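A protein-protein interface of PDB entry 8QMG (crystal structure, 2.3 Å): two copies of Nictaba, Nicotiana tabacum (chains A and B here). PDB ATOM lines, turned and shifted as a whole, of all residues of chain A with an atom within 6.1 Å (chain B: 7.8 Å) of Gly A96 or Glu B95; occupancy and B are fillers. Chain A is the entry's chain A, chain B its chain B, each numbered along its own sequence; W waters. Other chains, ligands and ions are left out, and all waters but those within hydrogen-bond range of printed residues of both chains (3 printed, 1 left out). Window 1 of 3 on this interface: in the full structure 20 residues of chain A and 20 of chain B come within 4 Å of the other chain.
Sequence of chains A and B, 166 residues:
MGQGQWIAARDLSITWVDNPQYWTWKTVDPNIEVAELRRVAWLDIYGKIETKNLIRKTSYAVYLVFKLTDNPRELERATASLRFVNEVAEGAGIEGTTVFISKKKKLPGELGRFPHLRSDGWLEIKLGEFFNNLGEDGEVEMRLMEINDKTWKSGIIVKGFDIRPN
OG1 of Thr A98 is in hydrogen-bond range of OE2 of Glu B95 (2.7 Å).
The backbone NH (N) of Thr B97 lies within hydrogen-bond range of the backbone carbonyl oxygen (O) of Ala B80, at 2.6 Å.
The backbone NH (N) of Ala A80 sits at hydrogen-bond distance from the backbone carbonyl oxygen (O) of Thr A97, at 2.8 Å.
Among the printed residues, pairs that only touch across the chains: Thr A97 with Glu B95, Glu A95 with Thr B97, Gly A96 with Glu B95 and Glu A95 with Gly B96.
Of the printed residues of chain B, Thr A97 touches Glu B95 (3.2 Å).
Gly B91 touches none of the printed residues of chain A.
Of chain A, only Gly A96, Thr A97 and Thr A98 come within 4 Å of Glu B95.
Of the printed residues of chain A, Thr B97 touches Glu A95 (3.3 Å).
The nearest printed residue of chain B that does not touch Glu A95 is Glu B95 (5.8 Å).
Glu A95 touches Gly B96, and with the chains exchanged Gly A96 touches Glu B95.
Glu A95 touches Thr B97, and with the chains exchanged Thr A97 touches Glu B95.
Positions printed for both chains: 79, 80, 81, 82, 94, 95, 96 and 97.
Water W3 bridges O of Glu B87 (2.6 Å) and O of Thr A98 (2.7 Å).
Water W1 lies within hydrogen-bond range of the backbone carbonyl oxygen of Thr A98 (2.7 Å), the side-chain carboxylate of Glu B95 (3.1 Å) and the backbone NH of Ala B89 (3.3 Å).
Water W2 lies within hydrogen-bond range of O of Gly A96 (3.4 Å) and OE2 of Glu B95 (3.5 Å).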
ATOM      1  N   THR A  79      22.684  16.866 -38.238  1.00  0.00           N
ATOM      2  CA  THR A  79      23.183  16.950 -36.875  1.00  0.00           C
ATOM      3  C   THR A  79      24.419  17.841 -36.830  1.00  0.00           C
ATOM      4  O   THR A  79      25.426  17.539 -37.475  1.00  0.00           O
ATOM      5  CB  THR A  79      23.504  15.556 -36.333  1.00  0.00           C
ATOM      6  OG1 THR A  79      22.301  14.775 -36.275  1.00  0.00           O
ATOM      7  CG2 THR A  79      24.128  15.659 -34.933  1.00  0.00           C
ATOM      8  N   ALA A  80      24.337  18.935 -36.080  1.00  0.00           N
ATOM      9  CA  ALA A  80      25.476  19.801 -35.818  1.00  0.00           C
ATOM     10  C   ALA A  80      26.033  19.505 -34.428  1.00  0.00           C
ATOM     11  O   ALA A  80      25.295  19.168 -33.500  1.00  0.00           O
ATOM     12  CB  ALA A  80      25.078  21.274 -35.920  1.00  0.00           C
ATOM     13  N   SER A  81      27.349  19.642 -34.292  1.00  0.00           N
ATOM     14  CA  SER A  81      28.026  19.332 -33.041  1.00  0.00           C
ATOM     15  C   SER A  81      29.201  20.278 -32.859  1.00  0.00           C
ATOM     16  O   SER A  81      29.865  20.642 -33.830  1.00  0.00           O
ATOM     17  CB  SER A  81      28.504  17.874 -33.023  1.00  0.00           C
ATOM     18  OG  SER A  81      29.449  17.650 -31.989  1.00  0.00           O
ATOM     19  N   LEU A  82      29.439  20.678 -31.610  1.00  0.00           N
ATOM     20  CA  LEU A  82      30.600  21.475 -31.240  1.00  0.00           C
ATOM     21  C   LEU A  82      30.816  21.290 -29.745  1.00  0.00           C
ATOM     22  O   LEU A  82      29.884  21.499 -28.957  1.00  0.00           O
ATOM     23  CB  LEU A  82      30.396  22.952 -31.575  1.00  0.00           C
ATOM     24  CG  LEU A  82      31.616  23.840 -31.333  1.00  0.00           C
ATOM     25  CD1 LEU A  82      31.670  24.980 -32.361  1.00  0.00           C
ATOM     26  CD2 LEU A  82      31.627  24.407 -29.926  1.00  0.00           C
ATOM     27  N   ILE A  94      28.188  11.263 -30.006  1.00  0.00           N
ATOM     28  CA  ILE A  94      28.440  12.593 -30.549  1.00  0.00           C
ATOM     29  C   ILE A  94      27.705  13.651 -29.732  1.00  0.00           C
ATOM     30  O   ILE A  94      28.260  14.704 -29.408  1.00  0.00           O
ATOM     31  CB  ILE A  94      28.041  12.645 -32.032  1.00  0.00           C
ATOM     32  CG1 ILE A  94      28.852  11.624 -32.834  1.00  0.00           C
ATOM     33  CG2 ILE A  94      28.228  14.047 -32.586  1.00  0.00           C
ATOM     34  CD1 ILE A  94      30.357  11.820 -32.767  1.00  0.00           C
ATOM     35  N   GLU A  95      26.446  13.398 -29.402  1.00  0.00           N
ATOM     36  CA  GLU A  95      25.657  14.294 -28.557  1.00  0.00           C
ATOM     37  C   GLU A  95      25.548  15.689 -29.172  1.00  0.00           C
ATOM     38  O   GLU A  95      25.965  16.686 -28.584  1.00  0.00           O
ATOM     39  CB  GLU A  95      26.248  14.366 -27.145  1.00  0.00           C
ATOM     40  CG  GLU A  95      26.271  13.022 -26.432  1.00  0.00           C
ATOM     41  CD  GLU A  95      26.671  13.129 -24.976  1.00  0.00           C
ATOM     42  OE1 GLU A  95      27.381  14.088 -24.615  1.00  0.00           O
ATOM     43  OE2 GLU A  95      26.265  12.248 -24.194  1.00  0.00           O
ATOM     44  N   GLY A  96      24.944  15.738 -30.361  1.00  0.00           N
ATOM     45  CA  GLY A  96      24.756  16.961 -31.097  1.00  0.00           C
ATOM     46  C   GLY A  96      23.324  17.461 -31.053  1.00  0.00           C
ATOM     47  O   GLY A  96      22.503  17.030 -30.237  1.00  0.00           O
ATOM     48  N   THR A  97      23.026  18.391 -31.958  1.00  0.00           N
ATOM     49  CA  THR A  97      21.720  19.026 -32.050  1.00  0.00           C
ATOM     50  C   THR A  97      21.240  19.023 -33.497  1.00  0.00           C
ATOM     51  O   THR A  97      22.036  18.999 -34.432  1.00  0.00           O
ATOM     52  CB  THR A  97      21.777  20.466 -31.527  1.00  0.00           C
ATOM     53  OG1 THR A  97      22.471  21.288 -32.469  1.00  0.00           O
ATOM     54  CG2 THR A  97      22.507  20.517 -30.193  1.00  0.00           C
ATOM     55  N   THR A  98      19.925  19.033 -33.670  1.00  0.00           N
ATOM     56  CA  THR A  98      19.316  18.978 -34.990  1.00  0.00           C
ATOM     57  C   THR A  98      19.205  20.384 -35.563  1.00  0.00           C
ATOM     58  O   THR A  98      18.673  21.288 -34.909  1.00  0.00           O
ATOM     59  CB  THR A  98      17.932  18.332 -34.932  1.00  0.00           C
ATOM     60  OG1 THR A  98      18.037  16.999 -34.420  1.00  0.00           O
ATOM     61  CG2 THR A  98      17.323  18.293 -36.329  1.00  0.00           C
ATOM     62  N   THR B  79      22.293  14.035 -17.648  1.00  0.00           N
ATOM     63  CA  THR B  79      22.198  14.729 -18.926  1.00  0.00           C
ATOM     64  C   THR B  79      21.989  16.214 -18.665  1.00  0.00           C
ATOM     65  O   THR B  79      21.042  16.596 -17.968  1.00  0.00           O
ATOM     66  CB  THR B  79      21.051  14.174 -19.772  1.00  0.00           C
ATOM     67  OG1 THR B  79      21.286  12.795 -20.057  1.00  0.00           O
ATOM     68  CG2 THR B  79      20.932  14.938 -21.079  1.00  0.00           C
ATOM     69  N   ALA B  80      22.880  17.040 -19.208  1.00  0.00           N
ATOM     70  CA  ALA B  80      22.757  18.489 -19.166  1.00  0.00           C
ATOM     71  C   ALA B  80      22.380  18.987 -20.550  1.00  0.00           C
ATOM     72  O   ALA B  80      22.886  18.481 -21.555  1.00  0.00           O
ATOM     73  CB  ALA B  80      24.059  19.150 -18.709  1.00  0.00           C
ATOM     74  N   SER B  81      21.484  19.972 -20.600  1.00  0.00           N
ATOM     75  CA  SER B  81      21.065  20.563 -21.859  1.00  0.00           C
ATOM     76  C   SER B  81      20.923  22.066 -21.698  1.00  0.00           C
ATOM     77  O   SER B  81      20.482  22.546 -20.652  1.00  0.00           O
ATOM     78  CB  SER B  81      19.736  19.980 -22.356  1.00  0.00           C
ATOM     79  OG  SER B  81      19.351  20.601 -23.578  1.00  0.00           O
ATOM     80  N   LEU B  82      21.312  22.801 -22.734  1.00  0.00           N
ATOM     81  CA  LEU B  82      21.107  24.242 -22.808  1.00  0.00           C
ATOM     82  C   LEU B  82      20.942  24.603 -24.277  1.00  0.00           C
ATOM     83  O   LEU B  82      21.786  24.244 -25.103  1.00  0.00           O
ATOM     84  CB  LEU B  82      22.277  25.009 -22.183  1.00  0.00           C
ATOM     85  CG  LEU B  82      22.090  26.532 -22.212  1.00  0.00           C
ATOM     86  CD1 LEU B  82      22.676  27.161 -20.971  1.00  0.00           C
ATOM     87  CD2 LEU B  82      22.731  27.112 -23.467  1.00  0.00           C
ATOM     88  N   ARG B  83      19.874  25.326 -24.598  1.00  0.00           N
ATOM     89  CA  ARG B  83      19.591  25.651 -25.989  1.00  0.00           C
ATOM     90  C   ARG B  83      18.650  26.841 -26.056  1.00  0.00           C
ATOM     91  O   ARG B  83      17.856  27.077 -25.141  1.00  0.00           O
ATOM     92  CB  ARG B  83      18.981  24.444 -26.715  1.00  0.00           C
ATOM     93  CG  ARG B  83      17.715  23.909 -26.063  1.00  0.00           C
ATOM     94  CD  ARG B  83      17.299  22.572 -26.660  1.00  0.00           C
ATOM     95  NE  ARG B  83      15.986  22.152 -26.181  1.00  0.00           N
ATOM     96  CZ  ARG B  83      15.331  21.097 -26.640  1.00  0.00           C
ATOM     97  NH1 ARG B  83      15.850  20.315 -27.573  1.00  0.00           N
ATOM     98  NH2 ARG B  83      14.125  20.820 -26.150  1.00  0.00           N
ATOM     99  N   GLU B  87      15.498  27.838 -31.306  1.00  0.00           N
ATOM    100  CA  GLU B  87      16.368  27.061 -32.176  1.00  0.00           C
ATOM    101  C   GLU B  87      16.097  25.565 -32.095  1.00  0.00           C
ATOM    102  O   GLU B  87      16.853  24.775 -32.671  1.00  0.00           O
ATOM    103  CB  GLU B  87      17.834  27.336 -31.842  1.00  0.00           C
ATOM    104  CG  GLU B  87      18.304  28.740 -32.196  1.00  0.00           C
ATOM    105  CD  GLU B  87      19.802  28.935 -31.996  1.00  0.00           C
ATOM    106  OE1 GLU B  87      20.466  28.007 -31.484  1.00  0.00           O
ATOM    107  OE2 GLU B  87      20.313  30.020 -32.348  1.00  0.00           O
ATOM    108  N   VAL B  88      15.054  25.158 -31.388  1.00  0.00           N
ATOM    109  CA  VAL B  88      14.713  23.747 -31.246  1.00  0.00           C
ATOM    110  C   VAL B  88      13.830  23.338 -32.418  1.00  0.00           C
ATOM    111  O   VAL B  88      12.722  23.859 -32.581  1.00  0.00           O
ATOM    112  CB  VAL B  88      14.010  23.482 -29.906  1.00  0.00           C
ATOM    113  CG1 VAL B  88      13.613  22.022 -29.799  1.00  0.00           C
ATOM    114  CG2 VAL B  88      14.911  23.893 -28.750  1.00  0.00           C
ATOM    115  N   ALA B  89      14.324  22.419 -33.239  1.00  0.00           N
ATOM    116  CA  ALA B  89      13.583  21.972 -34.408  1.00  0.00           C
ATOM    117  C   ALA B  89      12.397  21.113 -33.991  1.00  0.00           C
ATOM    118  O   ALA B  89      12.455  20.374 -33.007  1.00  0.00           O
ATOM    119  CB  ALA B  89      14.493  21.175 -35.339  1.00  0.00           C
ATOM    120  N   GLY B  91       9.953  18.308 -33.355  1.00  0.00           N
ATOM    121  CA  GLY B  91      10.145  16.886 -33.215  1.00  0.00           C
ATOM    122  C   GLY B  91      11.441  16.480 -32.549  1.00  0.00           C
ATOM    123  O   GLY B  91      11.573  15.324 -32.125  1.00  0.00           O
ATOM    124  N   ALA B  92      12.407  17.382 -32.465  1.00  0.00           N
ATOM    125  CA  ALA B  92      13.647  17.084 -31.768  1.00  0.00           C
ATOM    126  C   ALA B  92      13.391  16.970 -30.277  1.00  0.00           C
ATOM    127  O   ALA B  92      12.595  17.724 -29.709  1.00  0.00           O
ATOM    128  CB  ALA B  92      14.683  18.172 -32.032  1.00  0.00           C
ATOM    129  N   GLY B  93      14.072  16.029 -29.642  1.00  0.00           N
ATOM    130  CA  GLY B  93      13.935  15.829 -28.217  1.00  0.00           C
ATOM    131  C   GLY B  93      14.818  16.783 -27.440  1.00  0.00           C
ATOM    132  O   GLY B  93      15.262  17.816 -27.943  1.00  0.00           O
ATOM    133  N   ILE B  94      15.062  16.432 -26.182  1.00  0.00           N
ATOM    134  CA  ILE B  94      16.040  17.138 -25.363  1.00  0.00           C
ATOM    135  C   ILE B  94      17.414  16.642 -25.800  1.00  0.00           C
ATOM    136  O   ILE B  94      17.785  15.498 -25.533  1.00  0.00           O
ATOM    137  CB  ILE B  94      15.805  16.903 -23.868  1.00  0.00           C
ATOM    138  CG1 ILE B  94      14.411  17.408 -23.478  1.00  0.00           C
ATOM    139  CG2 ILE B  94      16.881  17.604 -23.052  1.00  0.00           C
ATOM    140  CD1 ILE B  94      13.949  16.960 -22.101  1.00  0.00           C
ATOM    141  N   GLU B  95      18.163  17.494 -26.477  1.00  0.00           N
ATOM    142  CA  GLU B  95      19.451  17.120 -27.058  1.00  0.00           C
ATOM    143  C   GLU B  95      20.544  17.702 -26.166  1.00  0.00           C
ATOM    144  O   GLU B  95      21.019  18.819 -26.384  1.00  0.00           O
ATOM    145  CB  GLU B  95      19.546  17.619 -28.499  1.00  0.00           C
ATOM    146  CG  GLU B  95      18.430  17.111 -29.384  1.00  0.00           C
ATOM    147  CD  GLU B  95      18.469  17.659 -30.796  1.00  0.00           C
ATOM    148  OE1 GLU B  95      18.701  18.872 -30.959  1.00  0.00           O
ATOM    149  OE2 GLU B  95      18.254  16.870 -31.740  1.00  0.00           O
ATOM    150  N   GLY B  96      20.928  16.934 -25.152  1.00  0.00           N
ATOM    151  CA  GLY B  96      21.892  17.379 -24.160  1.00  0.00           C
ATOM    152  C   GLY B  96      23.213  16.643 -24.248  1.00  0.00           C
ATOM    153  O   GLY B  96      23.501  15.900 -25.189  1.00  0.00           O
ATOM    154  N   THR B  97      24.032  16.865 -23.218  1.00  0.00           N
ATOM    155  CA  THR B  97      25.348  16.258 -23.114  1.00  0.00           C
ATOM    156  C   THR B  97      25.469  15.528 -21.781  1.00  0.00           C
ATOM    157  O   THR B  97      24.842  15.902 -20.790  1.00  0.00           O
ATOM    158  CB  THR B  97      26.474  17.304 -23.231  1.00  0.00           C
ATOM    159  OG1 THR B  97      26.455  18.151 -22.082  1.00  0.00           O
ATOM    160  CG2 THR B  97      26.280  18.162 -24.462  1.00  0.00           C
ATOM    161  N   ARG B 143      18.498  22.401 -18.438  1.00  0.00           N
ATOM    162  CA  ARG B 143      18.030  21.411 -17.484  1.00  0.00           C
ATOM    163  C   ARG B 143      19.122  20.390 -17.219  1.00  0.00           C
ATOM    164  O   ARG B 143      20.039  20.206 -18.021  1.00  0.00           O
ATOM    165  CB  ARG B 143      16.773  20.706 -17.998  1.00  0.00           C
ATOM    166  CG  ARG B 143      17.026  19.764 -19.173  1.00  0.00           C
ATOM    167  CD  ARG B 143      15.834  19.749 -20.121  1.00  0.00           C
ATOM    168  NE  ARG B 143      14.601  19.406 -19.428  1.00  0.00           N
ATOM    169  CZ  ARG B 143      13.386  19.649 -19.902  1.00  0.00           C
ATOM    170  NH1 ARG B 143      13.209  20.244 -21.068  1.00  0.00           N
ATOM    171  NH2 ARG B 143      12.325  19.287 -19.184  1.00  0.00           N
ATOM    172  N   MET B 145      18.877  16.262 -16.098  1.00  0.00           N
ATOM    173  CA  MET B 145      17.894  15.201 -15.941  1.00  0.00           C
ATOM    174  C   MET B 145      18.569  13.840 -15.960  1.00  0.00           C
ATOM    175  O   MET B 145      19.627  13.663 -16.562  1.00  0.00           O
ATOM    176  CB  MET B 145      16.822  15.278 -17.032  1.00  0.00           C
ATOM    177  CG  MET B 145      17.353  15.211 -18.443  1.00  0.00           C
ATOM    178  SD  MET B 145      16.160  15.868 -19.645  1.00  0.00           S
ATOM    179  CE  MET B 145      14.841  14.665 -19.516  1.00  0.00           C
HETATM  180  O   HOH W   1      17.238  21.015 -32.624  1.00  0.00           O
HETATM  181  O   HOH W   2      20.937  14.721 -32.243  1.00  0.00           O
HETATM  182  O   HOH W   3      17.522  23.699 -34.991  1.00  0.00           O
